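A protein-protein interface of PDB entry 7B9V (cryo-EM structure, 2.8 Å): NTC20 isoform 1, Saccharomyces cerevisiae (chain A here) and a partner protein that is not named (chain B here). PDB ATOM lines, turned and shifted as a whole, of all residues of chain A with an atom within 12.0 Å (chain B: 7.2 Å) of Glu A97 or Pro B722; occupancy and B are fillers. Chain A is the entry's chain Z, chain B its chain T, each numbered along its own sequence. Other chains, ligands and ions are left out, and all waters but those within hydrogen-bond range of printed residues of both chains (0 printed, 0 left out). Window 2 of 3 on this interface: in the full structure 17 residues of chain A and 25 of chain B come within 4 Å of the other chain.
Among the printed residues, pairs that only touch across the chains: Cys A96 with Thr B719, Cys A96 with Gly B721, Glu A97 with Gly B721 and Glu A97 with Pro B722.
O of Pro B722 is in hydrogen-bond range of NE of Arg B726 (3.0 Å).
N of Gly B721 sits at hydrogen-bond distance from O of Ala B716 (3.2 Å).
OG1 of Thr B725 sits at hydrogen-bond distance from O of Pro B722, at 2.9 Å.
The backbone carbonyl oxygen (O) of Cys A96 lies within hydrogen-bond range of the side-chain hydroxyl (OG) of Ser A99 (3.1 Å).
The side-chain hydroxyl (OG1) of Thr B725 is in hydrogen-bond range of the backbone carbonyl oxygen (O) of Gly B721.
Of the printed residues of chain B, Cys A96 touches Thr B719 (3.9 Å), Leu B720 (3.2 Å) and Gly B721 (3.998 Å).
Glu A97 touches just these residues of chain B: Leu B720, Gly B721, Pro B722 and Ser B723.
Asp A100 touches none of the printed residues of chain B.
Of the printed residues of chain A, Thr B719 touches Cys A96 and Ser A99.
Leu B720 touches two residues of chain A.
Of chain A, only Glu A97 comes within 4 Å of Pro B722.
Ser B723 touches one residue of chain A.
No residue of chain A comes within 4 Å of Val B724.
Arg B726 touches none of the printed residues of chain A.
Glu B727 touches none of the printed residues of chain A.
The nearest residue of chain A that does not touch Pro B722 is Cys A96 (4.9 Å).
OE1 of Glu A97 sits close to O of Leu B720 (3.4 Å).
O of Cys A96 sits close to O of Leu B720 (3.2 Å).
OG of Ser B723 is in hydrogen-bond range of OE1 of Glu A97 (2.7 Å).
The side-chain hydroxyl of Ser A99 is in hydrogen-bond range of the backbone carbonyl oxygen of Thr B719 (3.4 Å).
Of the 15 printed residues of chain B, 5 touch a printed residue of chain A.
Hydrophobic or aromatic side chains of chain B that line the printed part of chain A: Pro B722.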
ATOM      1  N   CYS A  96      26.742  20.236  29.202  1.00  0.00           N
ATOM      2  CA  CYS A  96      25.961  20.644  30.361  1.00  0.00           C
ATOM      3  C   CYS A  96      25.336  22.005  30.128  1.00  0.00           C
ATOM      4  O   CYS A  96      25.184  22.785  31.072  1.00  0.00           O
ATOM      5  CB  CYS A  96      26.856  20.705  31.602  1.00  0.00           C
ATOM      6  SG  CYS A  96      28.295  21.824  31.457  1.00  0.00           S
ATOM      7  N   GLU A  97      25.054  22.308  28.857  1.00  0.00           N
ATOM      8  CA  GLU A  97      24.611  23.648  28.491  1.00  0.00           C
ATOM      9  C   GLU A  97      23.245  24.009  29.061  1.00  0.00           C
ATOM     10  O   GLU A  97      22.969  25.184  29.321  1.00  0.00           O
ATOM     11  CB  GLU A  97      24.577  23.810  26.976  1.00  0.00           C
ATOM     12  CG  GLU A  97      25.951  23.759  26.293  1.00  0.00           C
ATOM     13  CD  GLU A  97      26.708  25.079  26.265  1.00  0.00           C
ATOM     14  OE1 GLU A  97      26.650  25.820  27.267  1.00  0.00           O
ATOM     15  OE2 GLU A  97      27.322  25.404  25.226  1.00  0.00           O
ATOM     16  N   THR A  98      22.385  23.014  29.255  1.00  0.00           N
ATOM     17  CA  THR A  98      21.014  23.217  29.702  1.00  0.00           C
ATOM     18  C   THR A  98      20.739  22.518  31.026  1.00  0.00           C
ATOM     19  O   THR A  98      19.601  22.110  31.269  1.00  0.00           O
ATOM     20  CB  THR A  98      20.018  22.728  28.649  1.00  0.00           C
ATOM     21  OG1 THR A  98      20.142  21.308  28.503  1.00  0.00           O
ATOM     22  CG2 THR A  98      20.241  23.403  27.302  1.00  0.00           C
ATOM     23  N   SER A  99      21.782  22.297  31.844  1.00  0.00           N
ATOM     24  CA  SER A  99      21.600  21.588  33.113  1.00  0.00           C
ATOM     25  C   SER A  99      20.682  22.340  34.074  1.00  0.00           C
ATOM     26  O   SER A  99      20.013  21.707  34.903  1.00  0.00           O
ATOM     27  CB  SER A  99      22.956  21.341  33.777  1.00  0.00           C
ATOM     28  OG  SER A  99      23.732  22.528  33.840  1.00  0.00           O
ATOM     29  N   ASP A 100      20.694  23.682  34.014  1.00  0.00           N
ATOM     30  CA  ASP A 100      19.879  24.494  34.916  1.00  0.00           C
ATOM     31  C   ASP A 100      18.386  24.245  34.698  1.00  0.00           C
ATOM     32  O   ASP A 100      17.618  24.133  35.659  1.00  0.00           O
ATOM     33  CB  ASP A 100      20.241  25.977  34.753  1.00  0.00           C
ATOM     34  CG  ASP A 100      20.046  26.485  33.324  1.00  0.00           C
ATOM     35  OD1 ASP A 100      20.461  25.775  32.382  1.00  0.00           O
ATOM     36  OD2 ASP A 100      19.453  27.570  33.140  1.00  0.00           O
ATOM     37  N   LEU A 101      17.960  24.158  33.432  1.00  0.00           N
ATOM     38  CA  LEU A 101      16.562  23.901  33.116  1.00  0.00           C
ATOM     39  C   LEU A 101      16.202  22.441  33.326  1.00  0.00           C
ATOM     40  O   LEU A 101      15.045  22.134  33.647  1.00  0.00           O
ATOM     41  CB  LEU A 101      16.250  24.310  31.681  1.00  0.00           C
ATOM     42  CG  LEU A 101      16.393  25.793  31.363  1.00  0.00           C
ATOM     43  CD1 LEU A 101      16.445  25.977  29.863  1.00  0.00           C
ATOM     44  CD2 LEU A 101      15.264  26.602  31.986  1.00  0.00           C
ATOM     45  N   LYS A 102      17.165  21.541  33.052  1.00  0.00           N
ATOM     46  CA  LYS A 102      16.984  20.115  33.310  1.00  0.00           C
ATOM     47  C   LYS A 102      16.693  19.860  34.781  1.00  0.00           C
ATOM     48  O   LYS A 102      15.848  19.018  35.117  1.00  0.00           O
ATOM     49  CB  LYS A 102      18.220  19.329  32.857  1.00  0.00           C
ATOM     50  CG  LYS A 102      18.059  17.809  32.971  1.00  0.00           C
ATOM     51  CD  LYS A 102      19.307  17.029  32.564  1.00  0.00           C
ATOM     52  CE  LYS A 102      19.624  17.177  31.084  1.00  0.00           C
ATOM     53  NZ  LYS A 102      20.763  16.306  30.678  1.00  0.00           N
ATOM     54  N   ALA A 103      17.415  20.558  35.670  1.00  0.00           N
ATOM     55  CA  ALA A 103      17.239  20.367  37.107  1.00  0.00           C
ATOM     56  C   ALA A 103      15.858  20.821  37.577  1.00  0.00           C
ATOM     57  O   ALA A 103      15.354  20.329  38.594  1.00  0.00           O
ATOM     58  CB  ALA A 103      18.327  21.119  37.871  1.00  0.00           C
ATOM     59  N   LYS A 104      15.244  21.765  36.862  1.00  0.00           N
ATOM     60  CA  LYS A 104      13.921  22.251  37.214  1.00  0.00           C
ATOM     61  C   LYS A 104      12.814  21.387  36.620  1.00  0.00           C
ATOM     62  O   LYS A 104      11.824  21.109  37.304  1.00  0.00           O
ATOM     63  CB  LYS A 104      13.748  23.717  36.776  1.00  0.00           C
ATOM     64  CG  LYS A 104      12.366  24.384  37.038  1.00  0.00           C
ATOM     65  CD  LYS A 104      11.806  24.200  38.475  1.00  0.00           C
ATOM     66  CE  LYS A 104      12.736  24.741  39.581  1.00  0.00           C
ATOM     67  NZ  LYS A 104      12.199  24.493  40.949  1.00  0.00           N
ATOM     68  N   ALA B 716      29.450  30.819  36.094  1.00  0.00           N
ATOM     69  CA  ALA B 716      29.277  30.462  34.690  1.00  0.00           C
ATOM     70  C   ALA B 716      30.106  29.240  34.320  1.00  0.00           C
ATOM     71  O   ALA B 716      29.586  28.289  33.723  1.00  0.00           O
ATOM     72  CB  ALA B 716      29.655  31.653  33.824  1.00  0.00           C
ATOM     73  N   GLU B 717      31.411  29.276  34.648  1.00  0.00           N
ATOM     74  CA  GLU B 717      32.307  28.173  34.315  1.00  0.00           C
ATOM     75  C   GLU B 717      31.922  26.903  35.055  1.00  0.00           C
ATOM     76  O   GLU B 717      32.008  25.805  34.496  1.00  0.00           O
ATOM     77  CB  GLU B 717      33.763  28.539  34.606  1.00  0.00           C
ATOM     78  CG  GLU B 717      34.385  29.515  33.615  1.00  0.00           C
ATOM     79  CD  GLU B 717      35.867  29.720  33.854  1.00  0.00           C
ATOM     80  OE1 GLU B 717      36.499  28.834  34.463  1.00  0.00           O
ATOM     81  OE2 GLU B 717      36.402  30.762  33.422  1.00  0.00           O
ATOM     82  N   THR B 719      28.889  25.991  36.405  1.00  0.00           N
ATOM     83  CA  THR B 719      27.534  25.486  36.242  1.00  0.00           C
ATOM     84  C   THR B 719      27.041  25.453  34.805  1.00  0.00           C
ATOM     85  O   THR B 719      26.482  24.444  34.365  1.00  0.00           O
ATOM     86  CB  THR B 719      26.571  26.335  37.087  1.00  0.00           C
ATOM     87  OG1 THR B 719      26.622  27.702  36.656  1.00  0.00           O
ATOM     88  CG2 THR B 719      26.939  26.256  38.558  1.00  0.00           C
ATOM     89  N   LEU B 720      27.226  26.537  34.061  1.00  0.00           N
ATOM     90  CA  LEU B 720      26.515  26.716  32.803  1.00  0.00           C
ATOM     91  C   LEU B 720      27.244  26.125  31.603  1.00  0.00           C
ATOM     92  O   LEU B 720      26.598  25.617  30.683  1.00  0.00           O
ATOM     93  CB  LEU B 720      26.205  28.190  32.588  1.00  0.00           C
ATOM     94  CG  LEU B 720      24.798  28.730  32.860  1.00  0.00           C
ATOM     95  CD1 LEU B 720      23.829  28.267  31.786  1.00  0.00           C
ATOM     96  CD2 LEU B 720      24.291  28.274  34.211  1.00  0.00           C
ATOM     97  N   GLY B 721      28.570  26.209  31.578  1.00  0.00           N
ATOM     98  CA  GLY B 721      29.366  25.570  30.558  1.00  0.00           C
ATOM     99  C   GLY B 721      29.775  26.535  29.464  1.00  0.00           C
ATOM    100  O   GLY B 721      29.728  27.751  29.669  1.00  0.00           O
ATOM    101  N   PRO B 722      30.177  26.015  28.290  1.00  0.00           N
ATOM    102  CA  PRO B 722      30.856  26.865  27.287  1.00  0.00           C
ATOM    103  C   PRO B 722      30.065  28.038  26.709  1.00  0.00           C
ATOM    104  O   PRO B 722      30.705  28.974  26.224  1.00  0.00           O
ATOM    105  CB  PRO B 722      31.217  25.861  26.178  1.00  0.00           C
ATOM    106  CG  PRO B 722      31.299  24.543  26.870  1.00  0.00           C
ATOM    107  CD  PRO B 722      30.216  24.593  27.914  1.00  0.00           C
ATOM    108  N   SER B 723      28.729  27.983  26.670  1.00  0.00           N
ATOM    109  CA  SER B 723      27.936  28.997  25.965  1.00  0.00           C
ATOM    110  C   SER B 723      28.052  30.385  26.577  1.00  0.00           C
ATOM    111  O   SER B 723      28.594  31.304  25.958  1.00  0.00           O
ATOM    112  CB  SER B 723      26.452  28.662  25.892  1.00  0.00           C
ATOM    113  OG  SER B 723      25.931  28.409  27.190  1.00  0.00           O
ATOM    114  N   VAL B 724      27.549  30.527  27.808  1.00  0.00           N
ATOM    115  CA  VAL B 724      27.421  31.861  28.378  1.00  0.00           C
ATOM    116  C   VAL B 724      28.776  32.366  28.878  1.00  0.00           C
ATOM    117  O   VAL B 724      28.947  33.581  28.993  1.00  0.00           O
ATOM    118  CB  VAL B 724      26.326  31.894  29.479  1.00  0.00           C
ATOM    119  CG1 VAL B 724      26.748  31.197  30.707  1.00  0.00           C
ATOM    120  CG2 VAL B 724      25.803  33.313  29.801  1.00  0.00           C
ATOM    121  N   THR B 725      29.723  31.460  29.224  1.00  0.00           N
ATOM    122  CA  THR B 725      31.082  31.872  29.602  1.00  0.00           C
ATOM    123  C   THR B 725      31.728  32.713  28.513  1.00  0.00           C
ATOM    124  O   THR B 725      32.331  33.755  28.792  1.00  0.00           O
ATOM    125  CB  THR B 725      31.956  30.649  29.872  1.00  0.00           C
ATOM    126  OG1 THR B 725      31.809  29.705  28.803  1.00  0.00           O
ATOM    127  CG2 THR B 725      31.588  30.006  31.165  1.00  0.00           C
ATOM    128  N   ARG B 726      31.667  32.233  27.269  1.00  0.00           N
ATOM    129  CA  ARG B 726      32.330  32.932  26.182  1.00  0.00           C
ATOM    130  C   ARG B 726      31.638  34.245  25.819  1.00  0.00           C
ATOM    131  O   ARG B 726      32.347  35.222  25.561  1.00  0.00           O
ATOM    132  CB  ARG B 726      32.418  31.976  24.984  1.00  0.00           C
ATOM    133  CG  ARG B 726      33.266  30.730  25.286  1.00  0.00           C
ATOM    134  CD  ARG B 726      33.427  29.791  24.102  1.00  0.00           C
ATOM    135  NE  ARG B 726      32.141  29.324  23.594  1.00  0.00           N
ATOM    136  CZ  ARG B 726      31.677  29.547  22.373  1.00  0.00           C
ATOM    137  NH1 ARG B 726      32.374  30.234  21.485  1.00  0.00           N
ATOM    138  NH2 ARG B 726      30.496  29.042  22.027  1.00  0.00           N
ATOM    139  N   GLU B 727      30.386  34.428  26.246  1.00  0.00           N
ATOM    140  CA  GLU B 727      29.694  35.696  26.063  1.00  0.00           C
ATOM    141  C   GLU B 727      29.839  36.632  27.247  1.00  0.00           C
ATOM    142  O   GLU B 727      29.629  37.836  27.087  1.00  0.00           O
ATOM    143  CB  GLU B 727      28.204  35.446  25.783  1.00  0.00           C
ATOM    144  CG  GLU B 727      27.932  34.775  24.439  1.00  0.00           C
ATOM    145  CD  GLU B 727      26.499  34.949  23.975  1.00  0.00           C
ATOM    146  OE1 GLU B 727      26.064  36.109  23.817  1.00  0.00           O
ATOM    147  OE2 GLU B 727      25.802  33.930  23.783  1.00  0.00           O
ATOM    148  N   PHE B 751      40.603  28.484  30.488  1.00  0.00           N
ATOM    149  CA  PHE B 751      39.327  27.798  30.280  1.00  0.00           C
ATOM    150  C   PHE B 751      39.202  27.270  28.852  1.00  0.00           C
ATOM    151  O   PHE B 751      38.804  26.114  28.634  1.00  0.00           O
ATOM    152  CB  PHE B 751      38.180  28.755  30.621  1.00  0.00           C
ATOM    153  CG  PHE B 751      36.811  28.165  30.427  1.00  0.00           C
ATOM    154  CD1 PHE B 751      36.388  27.088  31.195  1.00  0.00           C
ATOM    155  CD2 PHE B 751      35.934  28.709  29.497  1.00  0.00           C
ATOM    156  CE1 PHE B 751      35.125  26.544  31.018  1.00  0.00           C
ATOM    157  CE2 PHE B 751      34.669  28.175  29.317  1.00  0.00           C
ATOM    158  CZ  PHE B 751      34.264  27.091  30.078  1.00  0.00           C
ATOM    159  N   GLU B 752      39.502  28.136  27.866  1.00  0.00           N
ATOM    160  CA  GLU B 752      39.418  27.755  26.456  1.00  0.00           C
ATOM    161  C   GLU B 752      40.392  26.641  26.116  1.00  0.00           C
ATOM    162  O   GLU B 752      40.073  25.756  25.311  1.00  0.00           O
ATOM    163  CB  GLU B 752      39.672  28.956  25.550  1.00  0.00           C
ATOM    164  CG  GLU B 752      38.503  29.900  25.455  1.00  0.00           C
ATOM    165  CD  GLU B 752      37.431  29.449  24.479  1.00  0.00           C
ATOM    166  OE1 GLU B 752      36.532  28.686  24.891  1.00  0.00           O
ATOM    167  OE2 GLU B 752      37.472  29.878  23.307  1.00  0.00           O
ATOM    168  N   ILE B 755      39.106  23.436  27.255  1.00  0.00           N
ATOM    169  CA  ILE B 755      38.118  22.903  26.321  1.00  0.00           C
ATOM    170  C   ILE B 755      38.811  22.148  25.182  1.00  0.00           C
ATOM    171  O   ILE B 755      38.404  21.037  24.819  1.00  0.00           O
ATOM    172  CB  ILE B 755      37.178  24.031  25.836  1.00  0.00           C
ATOM    173  CG1 ILE B 755      36.205  24.405  26.957  1.00  0.00           C
ATOM    174  CG2 ILE B 755      36.385  23.640  24.604  1.00  0.00           C
ATOM    175  CD1 ILE B 755      35.438  25.684  26.721  1.00  0.00           C
ATOM    176  N   ARG B 760      42.159  28.421  19.224  1.00  0.00           N
ATOM    177  CA  ARG B 760      41.231  29.356  19.853  1.00  0.00           C
ATOM    178  C   ARG B 760      41.835  29.957  21.129  1.00  0.00           C
ATOM    179  O   ARG B 760      41.641  31.145  21.405  1.00  0.00           O
ATOM    180  CB  ARG B 760      39.867  28.660  20.095  1.00  0.00           C
ATOM    181  CG  ARG B 760      39.797  27.635  21.251  1.00  0.00           C
ATOM    182  CD  ARG B 760      38.668  26.662  21.262  1.00  0.00           C
ATOM    183  NE  ARG B 760      37.530  27.205  21.980  1.00  0.00           N
ATOM    184  CZ  ARG B 760      36.386  26.558  22.134  1.00  0.00           C
ATOM    185  NH1 ARG B 760      36.205  25.356  21.617  1.00  0.00           N
ATOM    186  NH2 ARG B 760      35.386  27.151  22.779  1.00  0.00           N
